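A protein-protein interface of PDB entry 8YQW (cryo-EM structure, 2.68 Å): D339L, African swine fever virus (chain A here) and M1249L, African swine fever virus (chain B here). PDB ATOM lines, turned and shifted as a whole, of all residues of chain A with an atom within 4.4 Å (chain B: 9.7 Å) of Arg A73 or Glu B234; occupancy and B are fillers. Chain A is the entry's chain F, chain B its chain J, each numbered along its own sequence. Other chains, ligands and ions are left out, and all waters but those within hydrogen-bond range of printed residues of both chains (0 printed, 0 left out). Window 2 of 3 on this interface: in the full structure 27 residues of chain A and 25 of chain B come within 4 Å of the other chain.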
ATOM      1  N   ILE A   6      10.147 -31.344 -10.025  1.00  0.00           N
ATOM      2  CA  ILE A   6       9.393 -30.216  -9.491  1.00  0.00           C
ATOM      3  C   ILE A   6       7.914 -30.568  -9.530  1.00  0.00           C
ATOM      4  O   ILE A   6       7.385 -30.925 -10.588  1.00  0.00           O
ATOM      5  CB  ILE A   6       9.674 -28.922 -10.275  1.00  0.00           C
ATOM      6  CG1 ILE A   6      11.131 -28.501 -10.083  1.00  0.00           C
ATOM      7  CG2 ILE A   6       8.746 -27.814  -9.820  1.00  0.00           C
ATOM      8  CD1 ILE A   6      11.505 -27.247 -10.822  1.00  0.00           C
ATOM      9  N   PHE A   7       7.253 -30.468  -8.380  1.00  0.00           N
ATOM     10  CA  PHE A   7       5.849 -30.813  -8.243  1.00  0.00           C
ATOM     11  C   PHE A   7       5.043 -29.586  -7.849  1.00  0.00           C
ATOM     12  O   PHE A   7       5.572 -28.631  -7.272  1.00  0.00           O
ATOM     13  CB  PHE A   7       5.627 -31.899  -7.186  1.00  0.00           C
ATOM     14  CG  PHE A   7       6.388 -33.165  -7.431  1.00  0.00           C
ATOM     15  CD1 PHE A   7       7.708 -33.281  -7.037  1.00  0.00           C
ATOM     16  CD2 PHE A   7       5.774 -34.250  -8.026  1.00  0.00           C
ATOM     17  CE1 PHE A   7       8.403 -34.447  -7.250  1.00  0.00           C
ATOM     18  CE2 PHE A   7       6.467 -35.417  -8.240  1.00  0.00           C
ATOM     19  CZ  PHE A   7       7.782 -35.516  -7.849  1.00  0.00           C
ATOM     20  N   GLU A   8       3.753 -29.631  -8.162  1.00  0.00           N
ATOM     21  CA  GLU A   8       2.783 -28.641  -7.723  1.00  0.00           C
ATOM     22  C   GLU A   8       1.703 -29.337  -6.916  1.00  0.00           C
ATOM     23  O   GLU A   8       1.233 -30.413  -7.294  1.00  0.00           O
ATOM     24  CB  GLU A   8       2.141 -27.923  -8.901  1.00  0.00           C
ATOM     25  CG  GLU A   8       3.067 -27.030  -9.674  1.00  0.00           C
ATOM     26  CD  GLU A   8       2.331 -26.242 -10.725  1.00  0.00           C
ATOM     27  OE1 GLU A   8       1.119 -26.485 -10.909  1.00  0.00           O
ATOM     28  OE2 GLU A   8       2.957 -25.386 -11.372  1.00  0.00           O
ATOM     29  N   VAL A  51      11.231 -25.500  -1.516  1.00  0.00           N
ATOM     30  CA  VAL A  51      10.020 -24.875  -2.035  1.00  0.00           C
ATOM     31  C   VAL A  51      10.451 -23.728  -2.938  1.00  0.00           C
ATOM     32  O   VAL A  51      10.969 -22.714  -2.453  1.00  0.00           O
ATOM     33  CB  VAL A  51       9.106 -24.372  -0.909  1.00  0.00           C
ATOM     34  CG1 VAL A  51       7.940 -23.583  -1.480  1.00  0.00           C
ATOM     35  CG2 VAL A  51       8.613 -25.533  -0.065  1.00  0.00           C
ATOM     36  N   ILE A  52      10.245 -23.880  -4.249  1.00  0.00           N
ATOM     37  CA  ILE A  52      10.657 -22.835  -5.181  1.00  0.00           C
ATOM     38  C   ILE A  52       9.813 -21.585  -4.978  1.00  0.00           C
ATOM     39  O   ILE A  52      10.339 -20.473  -4.853  1.00  0.00           O
ATOM     40  CB  ILE A  52      10.566 -23.336  -6.633  1.00  0.00           C
ATOM     41  CG1 ILE A  52      11.525 -24.501  -6.866  1.00  0.00           C
ATOM     42  CG2 ILE A  52      10.859 -22.208  -7.604  1.00  0.00           C
ATOM     43  CD1 ILE A  52      10.856 -25.838  -6.798  1.00  0.00           C
ATOM     44  N   GLN A  53       8.494 -21.747  -4.939  1.00  0.00           N
ATOM     45  CA  GLN A  53       7.597 -20.628  -4.700  1.00  0.00           C
ATOM     46  C   GLN A  53       6.245 -21.172  -4.271  1.00  0.00           C
ATOM     47  O   GLN A  53       5.887 -22.309  -4.581  1.00  0.00           O
ATOM     48  CB  GLN A  53       7.467 -19.737  -5.936  1.00  0.00           C
ATOM     49  CG  GLN A  53       6.851 -20.403  -7.140  1.00  0.00           C
ATOM     50  CD  GLN A  53       7.004 -19.557  -8.383  1.00  0.00           C
ATOM     51  OE1 GLN A  53       7.675 -18.529  -8.366  1.00  0.00           O
ATOM     52  NE2 GLN A  53       6.374 -19.978  -9.465  1.00  0.00           N
ATOM     53  N   HIS A  71      -1.120 -23.106  -2.304  1.00  0.00           N
ATOM     54  CA  HIS A  71      -0.494 -23.760  -3.442  1.00  0.00           C
ATOM     55  C   HIS A  71       1.018 -23.749  -3.262  1.00  0.00           C
ATOM     56  O   HIS A  71       1.611 -22.697  -3.009  1.00  0.00           O
ATOM     57  CB  HIS A  71      -0.879 -23.061  -4.744  1.00  0.00           C
ATOM     58  CG  HIS A  71      -2.350 -22.833  -4.901  1.00  0.00           C
ATOM     59  ND1 HIS A  71      -3.269 -23.859  -4.881  1.00  0.00           N
ATOM     60  CD2 HIS A  71      -3.060 -21.698  -5.092  1.00  0.00           C
ATOM     61  CE1 HIS A  71      -4.481 -23.365  -5.048  1.00  0.00           C
ATOM     62  NE2 HIS A  71      -4.381 -22.055  -5.179  1.00  0.00           N
ATOM     63  N   VAL A  72       1.640 -24.916  -3.387  1.00  0.00           N
ATOM     64  CA  VAL A  72       3.070 -25.079  -3.163  1.00  0.00           C
ATOM     65  C   VAL A  72       3.694 -25.682  -4.412  1.00  0.00           C
ATOM     66  O   VAL A  72       3.213 -26.698  -4.928  1.00  0.00           O
ATOM     67  CB  VAL A  72       3.358 -25.960  -1.934  1.00  0.00           C
ATOM     68  CG1 VAL A  72       4.842 -25.972  -1.631  1.00  0.00           C
ATOM     69  CG2 VAL A  72       2.575 -25.473  -0.735  1.00  0.00           C
ATOM     70  N   ARG A  73       4.762 -25.057  -4.890  1.00  0.00           N
ATOM     71  CA  ARG A  73       5.563 -25.562  -5.999  1.00  0.00           C
ATOM     72  C   ARG A  73       6.926 -25.925  -5.425  1.00  0.00           C
ATOM     73  O   ARG A  73       7.722 -25.038  -5.099  1.00  0.00           O
ATOM     74  CB  ARG A  73       5.668 -24.517  -7.106  1.00  0.00           C
ATOM     75  CG  ARG A  73       6.421 -24.956  -8.340  1.00  0.00           C
ATOM     76  CD  ARG A  73       6.303 -23.908  -9.430  1.00  0.00           C
ATOM     77  NE  ARG A  73       5.008 -23.940 -10.097  1.00  0.00           N
ATOM     78  CZ  ARG A  73       4.558 -22.997 -10.915  1.00  0.00           C
ATOM     79  NH1 ARG A  73       5.252 -21.900 -11.153  1.00  0.00           N
ATOM     80  NH2 ARG A  73       3.383 -23.160 -11.512  1.00  0.00           N
ATOM     81  N   PHE A  74       7.190 -27.220  -5.284  1.00  0.00           N
ATOM     82  CA  PHE A  74       8.332 -27.679  -4.506  1.00  0.00           C
ATOM     83  C   PHE A  74       9.205 -28.636  -5.303  1.00  0.00           C
ATOM     84  O   PHE A  74       8.724 -29.400  -6.142  1.00  0.00           O
ATOM     85  CB  PHE A  74       7.881 -28.346  -3.195  1.00  0.00           C
ATOM     86  CG  PHE A  74       7.131 -29.634  -3.385  1.00  0.00           C
ATOM     87  CD1 PHE A  74       5.779 -29.628  -3.676  1.00  0.00           C
ATOM     88  CD2 PHE A  74       7.774 -30.851  -3.248  1.00  0.00           C
ATOM     89  CE1 PHE A  74       5.089 -30.807  -3.841  1.00  0.00           C
ATOM     90  CE2 PHE A  74       7.088 -32.032  -3.415  1.00  0.00           C
ATOM     91  CZ  PHE A  74       5.744 -32.010  -3.709  1.00  0.00           C
ATOM     92  N   MET B 143       6.071 -27.092 -22.142  1.00  0.00           N
ATOM     93  CA  MET B 143       6.054 -26.391 -20.862  1.00  0.00           C
ATOM     94  C   MET B 143       4.824 -26.762 -20.047  1.00  0.00           C
ATOM     95  O   MET B 143       4.918 -26.972 -18.835  1.00  0.00           O
ATOM     96  CB  MET B 143       6.112 -24.881 -21.083  1.00  0.00           C
ATOM     97  CG  MET B 143       7.463 -24.378 -21.546  1.00  0.00           C
ATOM     98  SD  MET B 143       8.746 -24.700 -20.326  1.00  0.00           S
ATOM     99  CE  MET B 143       9.588 -26.071 -21.103  1.00  0.00           C
ATOM    100  N   ARG B 144       3.662 -26.847 -20.694  1.00  0.00           N
ATOM    101  CA  ARG B 144       2.444 -27.225 -19.988  1.00  0.00           C
ATOM    102  C   ARG B 144       2.520 -28.660 -19.479  1.00  0.00           C
ATOM    103  O   ARG B 144       2.080 -28.951 -18.361  1.00  0.00           O
ATOM    104  CB  ARG B 144       1.236 -27.035 -20.903  1.00  0.00           C
ATOM    105  CG  ARG B 144      -0.070 -26.799 -20.170  1.00  0.00           C
ATOM    106  CD  ARG B 144      -1.188 -26.486 -21.149  1.00  0.00           C
ATOM    107  NE  ARG B 144      -2.482 -26.365 -20.490  1.00  0.00           N
ATOM    108  CZ  ARG B 144      -3.641 -26.303 -21.131  1.00  0.00           C
ATOM    109  NH1 ARG B 144      -3.703 -26.344 -22.452  1.00  0.00           N
ATOM    110  NH2 ARG B 144      -4.765 -26.201 -20.430  1.00  0.00           N
ATOM    111  N   ALA B 146       5.266 -30.334 -18.691  1.00  0.00           N
ATOM    112  CA  ALA B 146       6.176 -30.332 -17.550  1.00  0.00           C
ATOM    113  C   ALA B 146       5.540 -29.667 -16.336  1.00  0.00           C
ATOM    114  O   ALA B 146       5.830 -30.046 -15.196  1.00  0.00           O
ATOM    115  CB  ALA B 146       7.484 -29.637 -17.920  1.00  0.00           C
ATOM    116  N   GLU B 147       4.682 -28.671 -16.567  1.00  0.00           N
ATOM    117  CA  GLU B 147       3.925 -28.055 -15.485  1.00  0.00           C
ATOM    118  C   GLU B 147       3.017 -29.074 -14.813  1.00  0.00           C
ATOM    119  O   GLU B 147       2.930 -29.123 -13.581  1.00  0.00           O
ATOM    120  CB  GLU B 147       3.101 -26.877 -16.010  1.00  0.00           C
ATOM    121  CG  GLU B 147       3.935 -25.697 -16.482  1.00  0.00           C
ATOM    122  CD  GLU B 147       3.086 -24.580 -17.061  1.00  0.00           C
ATOM    123  OE1 GLU B 147       1.875 -24.799 -17.268  1.00  0.00           O
ATOM    124  OE2 GLU B 147       3.632 -23.485 -17.310  1.00  0.00           O
ATOM    125  N   ILE B 148       2.332 -29.894 -15.611  1.00  0.00           N
ATOM    126  CA  ILE B 148       1.552 -30.996 -15.054  1.00  0.00           C
ATOM    127  C   ILE B 148       2.470 -31.978 -14.340  1.00  0.00           C
ATOM    128  O   ILE B 148       2.164 -32.453 -13.241  1.00  0.00           O
ATOM    129  CB  ILE B 148       0.728 -31.676 -16.161  1.00  0.00           C
ATOM    130  CG1 ILE B 148      -0.410 -30.761 -16.611  1.00  0.00           C
ATOM    131  CG2 ILE B 148       0.175 -32.997 -15.681  1.00  0.00           C
ATOM    132  CD1 ILE B 148      -1.042 -31.176 -17.913  1.00  0.00           C
ATOM    133  N   MET B 226      14.287 -26.884 -17.788  1.00  0.00           N
ATOM    134  CA  MET B 226      13.516 -25.857 -18.480  1.00  0.00           C
ATOM    135  C   MET B 226      12.491 -25.214 -17.554  1.00  0.00           C
ATOM    136  O   MET B 226      12.364 -23.982 -17.523  1.00  0.00           O
ATOM    137  CB  MET B 226      12.830 -26.437 -19.715  1.00  0.00           C
ATOM    138  CG  MET B 226      13.778 -26.787 -20.843  1.00  0.00           C
ATOM    139  SD  MET B 226      12.936 -27.200 -22.378  1.00  0.00           S
ATOM    140  CE  MET B 226      12.547 -25.563 -22.992  1.00  0.00           C
ATOM    141  N   VAL B 227      11.759 -26.022 -16.779  1.00  0.00           N
ATOM    142  CA  VAL B 227      10.776 -25.426 -15.882  1.00  0.00           C
ATOM    143  C   VAL B 227      11.467 -24.623 -14.786  1.00  0.00           C
ATOM    144  O   VAL B 227      10.987 -23.548 -14.404  1.00  0.00           O
ATOM    145  CB  VAL B 227       9.823 -26.497 -15.309  1.00  0.00           C
ATOM    146  CG1 VAL B 227      10.538 -27.436 -14.354  1.00  0.00           C
ATOM    147  CG2 VAL B 227       8.638 -25.837 -14.625  1.00  0.00           C
ATOM    148  N   HIS B 228      12.619 -25.090 -14.290  1.00  0.00           N
ATOM    149  CA  HIS B 228      13.316 -24.357 -13.239  1.00  0.00           C
ATOM    150  C   HIS B 228      13.870 -23.038 -13.763  1.00  0.00           C
ATOM    151  O   HIS B 228      13.842 -22.024 -13.056  1.00  0.00           O
ATOM    152  CB  HIS B 228      14.430 -25.224 -12.655  1.00  0.00           C
ATOM    153  CG  HIS B 228      14.868 -24.805 -11.286  1.00  0.00           C
ATOM    154  ND1 HIS B 228      16.049 -25.234 -10.720  1.00  0.00           N
ATOM    155  CD2 HIS B 228      14.278 -24.008 -10.365  1.00  0.00           C
ATOM    156  CE1 HIS B 228      16.171 -24.714  -9.511  1.00  0.00           C
ATOM    157  NE2 HIS B 228      15.109 -23.966  -9.272  1.00  0.00           N
ATOM    158  N   ARG B 229      14.373 -23.026 -15.001  1.00  0.00           N
ATOM    159  CA  ARG B 229      14.854 -21.783 -15.592  1.00  0.00           C
ATOM    160  C   ARG B 229      13.709 -20.812 -15.840  1.00  0.00           C
ATOM    161  O   ARG B 229      13.867 -19.602 -15.651  1.00  0.00           O
ATOM    162  CB  ARG B 229      15.609 -22.069 -16.889  1.00  0.00           C
ATOM    163  CG  ARG B 229      16.924 -22.807 -16.690  1.00  0.00           C
ATOM    164  CD  ARG B 229      17.710 -22.901 -17.985  1.00  0.00           C
ATOM    165  NE  ARG B 229      18.174 -21.595 -18.435  1.00  0.00           N
ATOM    166  CZ  ARG B 229      19.307 -21.031 -18.042  1.00  0.00           C
ATOM    167  NH1 ARG B 229      20.122 -21.634 -17.192  1.00  0.00           N
ATOM    168  NH2 ARG B 229      19.632 -19.830 -18.514  1.00  0.00           N
ATOM    169  N   LYS B 230      12.550 -21.319 -16.269  1.00  0.00           N
ATOM    170  CA  LYS B 230      11.385 -20.451 -16.413  1.00  0.00           C
ATOM    171  C   LYS B 230      10.995 -19.834 -15.074  1.00  0.00           C
ATOM    172  O   LYS B 230      10.731 -18.627 -14.988  1.00  0.00           O
ATOM    173  CB  LYS B 230      10.219 -21.238 -17.010  1.00  0.00           C
ATOM    174  CG  LYS B 230       8.841 -20.701 -16.656  1.00  0.00           C
ATOM    175  CD  LYS B 230       7.766 -21.736 -16.945  1.00  0.00           C
ATOM    176  CE  LYS B 230       6.414 -21.301 -16.409  1.00  0.00           C
ATOM    177  NZ  LYS B 230       6.460 -21.008 -14.951  1.00  0.00           N
ATOM    178  N   LEU B 231      10.980 -20.647 -14.012  1.00  0.00           N
ATOM    179  CA  LEU B 231      10.655 -20.132 -12.687  1.00  0.00           C
ATOM    180  C   LEU B 231      11.662 -19.085 -12.236  1.00  0.00           C
ATOM    181  O   LEU B 231      11.284 -18.042 -11.691  1.00  0.00           O
ATOM    182  CB  LEU B 231      10.597 -21.275 -11.674  1.00  0.00           C
ATOM    183  CG  LEU B 231       9.584 -22.382 -11.950  1.00  0.00           C
ATOM    184  CD1 LEU B 231       9.538 -23.372 -10.805  1.00  0.00           C
ATOM    185  CD2 LEU B 231       8.223 -21.789 -12.212  1.00  0.00           C
ATOM    186  N   ASP B 232      12.954 -19.347 -12.445  1.00  0.00           N
ATOM    187  CA  ASP B 232      13.978 -18.399 -12.018  1.00  0.00           C
ATOM    188  C   ASP B 232      13.894 -17.095 -12.800  1.00  0.00           C
ATOM    189  O   ASP B 232      14.043 -16.013 -12.222  1.00  0.00           O
ATOM    190  CB  ASP B 232      15.364 -19.028 -12.155  1.00  0.00           C
ATOM    191  CG  ASP B 232      15.737 -19.875 -10.954  1.00  0.00           C
ATOM    192  OD1 ASP B 232      15.124 -19.689  -9.882  1.00  0.00           O
ATOM    193  OD2 ASP B 232      16.644 -20.725 -11.078  1.00  0.00           O
ATOM    194  N   ARG B 233      13.655 -17.168 -14.113  1.00  0.00           N
ATOM    195  CA  ARG B 233      13.599 -15.943 -14.903  1.00  0.00           C
ATOM    196  C   ARG B 233      12.344 -15.135 -14.600  1.00  0.00           C
ATOM    197  O   ARG B 233      12.382 -13.901 -14.653  1.00  0.00           O
ATOM    198  CB  ARG B 233      13.701 -16.257 -16.399  1.00  0.00           C
ATOM    199  CG  ARG B 233      12.389 -16.584 -17.091  1.00  0.00           C
ATOM    200  CD  ARG B 233      12.631 -17.047 -18.519  1.00  0.00           C
ATOM    201  NE  ARG B 233      13.481 -18.229 -18.572  1.00  0.00           N
ATOM    202  CZ  ARG B 233      13.998 -18.729 -19.686  1.00  0.00           C
ATOM    203  NH1 ARG B 233      13.765 -18.177 -20.865  1.00  0.00           N
ATOM    204  NH2 ARG B 233      14.768 -19.811 -19.614  1.00  0.00           N
ATOM    205  N   GLU B 234      11.229 -15.794 -14.272  1.00  0.00           N
ATOM    206  CA  GLU B 234      10.063 -15.040 -13.829  1.00  0.00           C
ATOM    207  C   GLU B 234      10.140 -14.655 -12.357  1.00  0.00           C
ATOM    208  O   GLU B 234       9.303 -13.876 -11.892  1.00  0.00           O
ATOM    209  CB  GLU B 234       8.779 -15.835 -14.081  1.00  0.00           C
ATOM    210  CG  GLU B 234       8.544 -16.980 -13.109  1.00  0.00           C
ATOM    211  CD  GLU B 234       7.233 -17.702 -13.366  1.00  0.00           C
ATOM    212  OE1 GLU B 234       6.535 -17.343 -14.337  1.00  0.00           O
ATOM    213  OE2 GLU B 234       6.902 -18.624 -12.594  1.00  0.00           O
ATOM    214  N   ASP B 235      11.122 -15.178 -11.621  1.00  0.00           N
ATOM    215  CA  ASP B 235      11.246 -14.962 -10.187  1.00  0.00           C
ATOM    216  C   ASP B 235      12.500 -14.173  -9.832  1.00  0.00           C
ATOM    217  O   ASP B 235      12.408 -13.112  -9.208  1.00  0.00           O
ATOM    218  CB  ASP B 235      11.239 -16.326  -9.479  1.00  0.00           C
ATOM    219  CG  ASP B 235      11.171 -16.214  -7.965  1.00  0.00           C
ATOM    220  OD1 ASP B 235      11.277 -15.094  -7.424  1.00  0.00           O
ATOM    221  OD2 ASP B 235      11.009 -17.268  -7.313  1.00  0.00           O
ATOM    222  N   GLN B 236      13.677 -14.662 -10.221  1.00  0.00           N
ATOM    223  CA  GLN B 236      14.934 -14.015  -9.862  1.00  0.00           C
ATOM    224  C   GLN B 236      15.318 -12.913 -10.841  1.00  0.00           C
ATOM    225  O   GLN B 236      15.794 -11.852 -10.424  1.00  0.00           O
ATOM    226  CB  GLN B 236      16.052 -15.059  -9.773  1.00  0.00           C
ATOM    227  CG  GLN B 236      17.426 -14.490  -9.451  1.00  0.00           C
ATOM    228  CD  GLN B 236      18.506 -15.558  -9.413  1.00  0.00           C
ATOM    229  OE1 GLN B 236      18.230 -16.744  -9.593  1.00  0.00           O
ATOM    230  NE2 GLN B 236      19.744 -15.138  -9.178  1.00  0.00           N
ATOM    231  N   GLY B 237      15.116 -13.141 -12.139  1.00  0.00           N
ATOM    232  CA  GLY B 237      15.362 -12.113 -13.130  1.00  0.00           C
ATOM    233  C   GLY B 237      14.297 -11.045 -13.213  1.00  0.00           C
ATOM    234  O   GLY B 237      14.506 -10.027 -13.882  1.00  0.00           O
ATOM    235  N   SER B 238      13.162 -11.255 -12.549  1.00  0.00           N
ATOM    236  CA  SER B 238      12.077 -10.283 -12.532  1.00  0.00           C
ATOM    237  C   SER B 238      11.684  -9.967 -11.096  1.00  0.00           C
ATOM    238  O   SER B 238      12.377 -10.370 -10.155  1.00  0.00           O
ATOM    239  CB  SER B 238      10.872 -10.810 -13.316  1.00  0.00           C
ATOM    240  OG  SER B 238      11.233 -11.136 -14.646  1.00  0.00           O
ATOM    241  N   HIS B 239      10.583  -9.246 -10.914  1.00  0.00           N
ATOM    242  CA  HIS B 239      10.108  -8.915  -9.575  1.00  0.00           C
ATOM    243  C   HIS B 239       8.584  -8.927  -9.511  1.00  0.00           C
ATOM    244  O   HIS B 239       7.961  -9.989  -9.525  1.00  0.00           O
ATOM    245  CB  HIS B 239      10.645  -7.551  -9.137  1.00  0.00           C
ATOM    246  CG  HIS B 239      10.278  -6.431 -10.060  1.00  0.00           C
ATOM    247  ND1 HIS B 239       9.059  -5.789 -10.003  1.00  0.00           N
ATOM    248  CD2 HIS B 239      10.970  -5.835 -11.059  1.00  0.00           C
ATOM    249  CE1 HIS B 239       9.016  -4.847 -10.929  1.00  0.00           C
ATOM    250  NE2 HIS B 239      10.163  -4.855 -11.584  1.00  0.00           N
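OE2 of Glu B234 is in hydrogen-bond range of NE2 of Gln A53 (3.5 Å). The side-chain carboxylate (OE2) of Glu B234 lies within salt-bridge range of the guanidinium group (NH1) of Arg A73 (3.9 Å).
NZ of Lys B230 lies within salt-bridge range of OE2 of Glu B234 (3.4 Å). OE2 of Glu A8 lies within salt-bridge range of NE of Arg A73 (2.8 Å). O of Arg A73 sits at hydrogen-bond distance from N of Ile A52 (2.9 Å). The guanidinium group (NH1) of Arg A73 sits close to the side-chain amide nitrogen (NE2) of Gln A53 (2.8 Å).
Among the printed residues, pairs that only touch across the chains: Ile A6 with Val B227 (3.7 Å), Ile A52 with Leu B231 (3.7 Å), Gln A53 with Leu B231 (3.8 Å), Gln A53 with Asp B235 (3.7 Å) and Arg A73 with Leu B231 (3.2 Å).
Arg A73 touches two residues of chain B. Of chain A, only Gln A53 and Arg A73 come within 4 Å of Glu B234. Val A51 touches none of the printed residues of chain B. Ile A52 touches just one residue of chain B: Leu B231. Gln A53 touches three residues of chain B. Printed residues of chain A within 4 Å of Val B227: Ile A6 (3.7 Å). Printed residues of chain B within 4 Å of Ile A6: Val B227 (3.7 Å). Of the printed residues of chain A, Asp B235 touches Gln A53 (3.7 Å). Printed residues of chain A within 4 Å of Leu B231: Ile A52 (3.7 Å), Gln A53 (3.8 Å) and Arg A73 (3.2 Å). His B239 touches none of the printed residues of chain A. Lys B230 touches none of the printed residues of chain A. The nearest residue of chain B that does not touch Arg A73 is Lys B230 (4.1 Å). The nearest printed residue of chain A that does not touch Glu B234 is Ile A52 (7.3 Å).
Hydrophobic or aromatic side chains of chain B within 4 Å of the printed part of chain A: Val B227 and Leu B231. Hydrophobic or aromatic side chains of chain A that line the printed part of chain B: Ile A6 and Ile A52. Among the printed residues, 7 pairs touch across the chains. Among the printed residues, Asp or Glu carboxylates within 4 Å of a Lys or Arg side-chain nitrogen of the other chain: Arg A73 with Glu B234 (3.9 Å).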
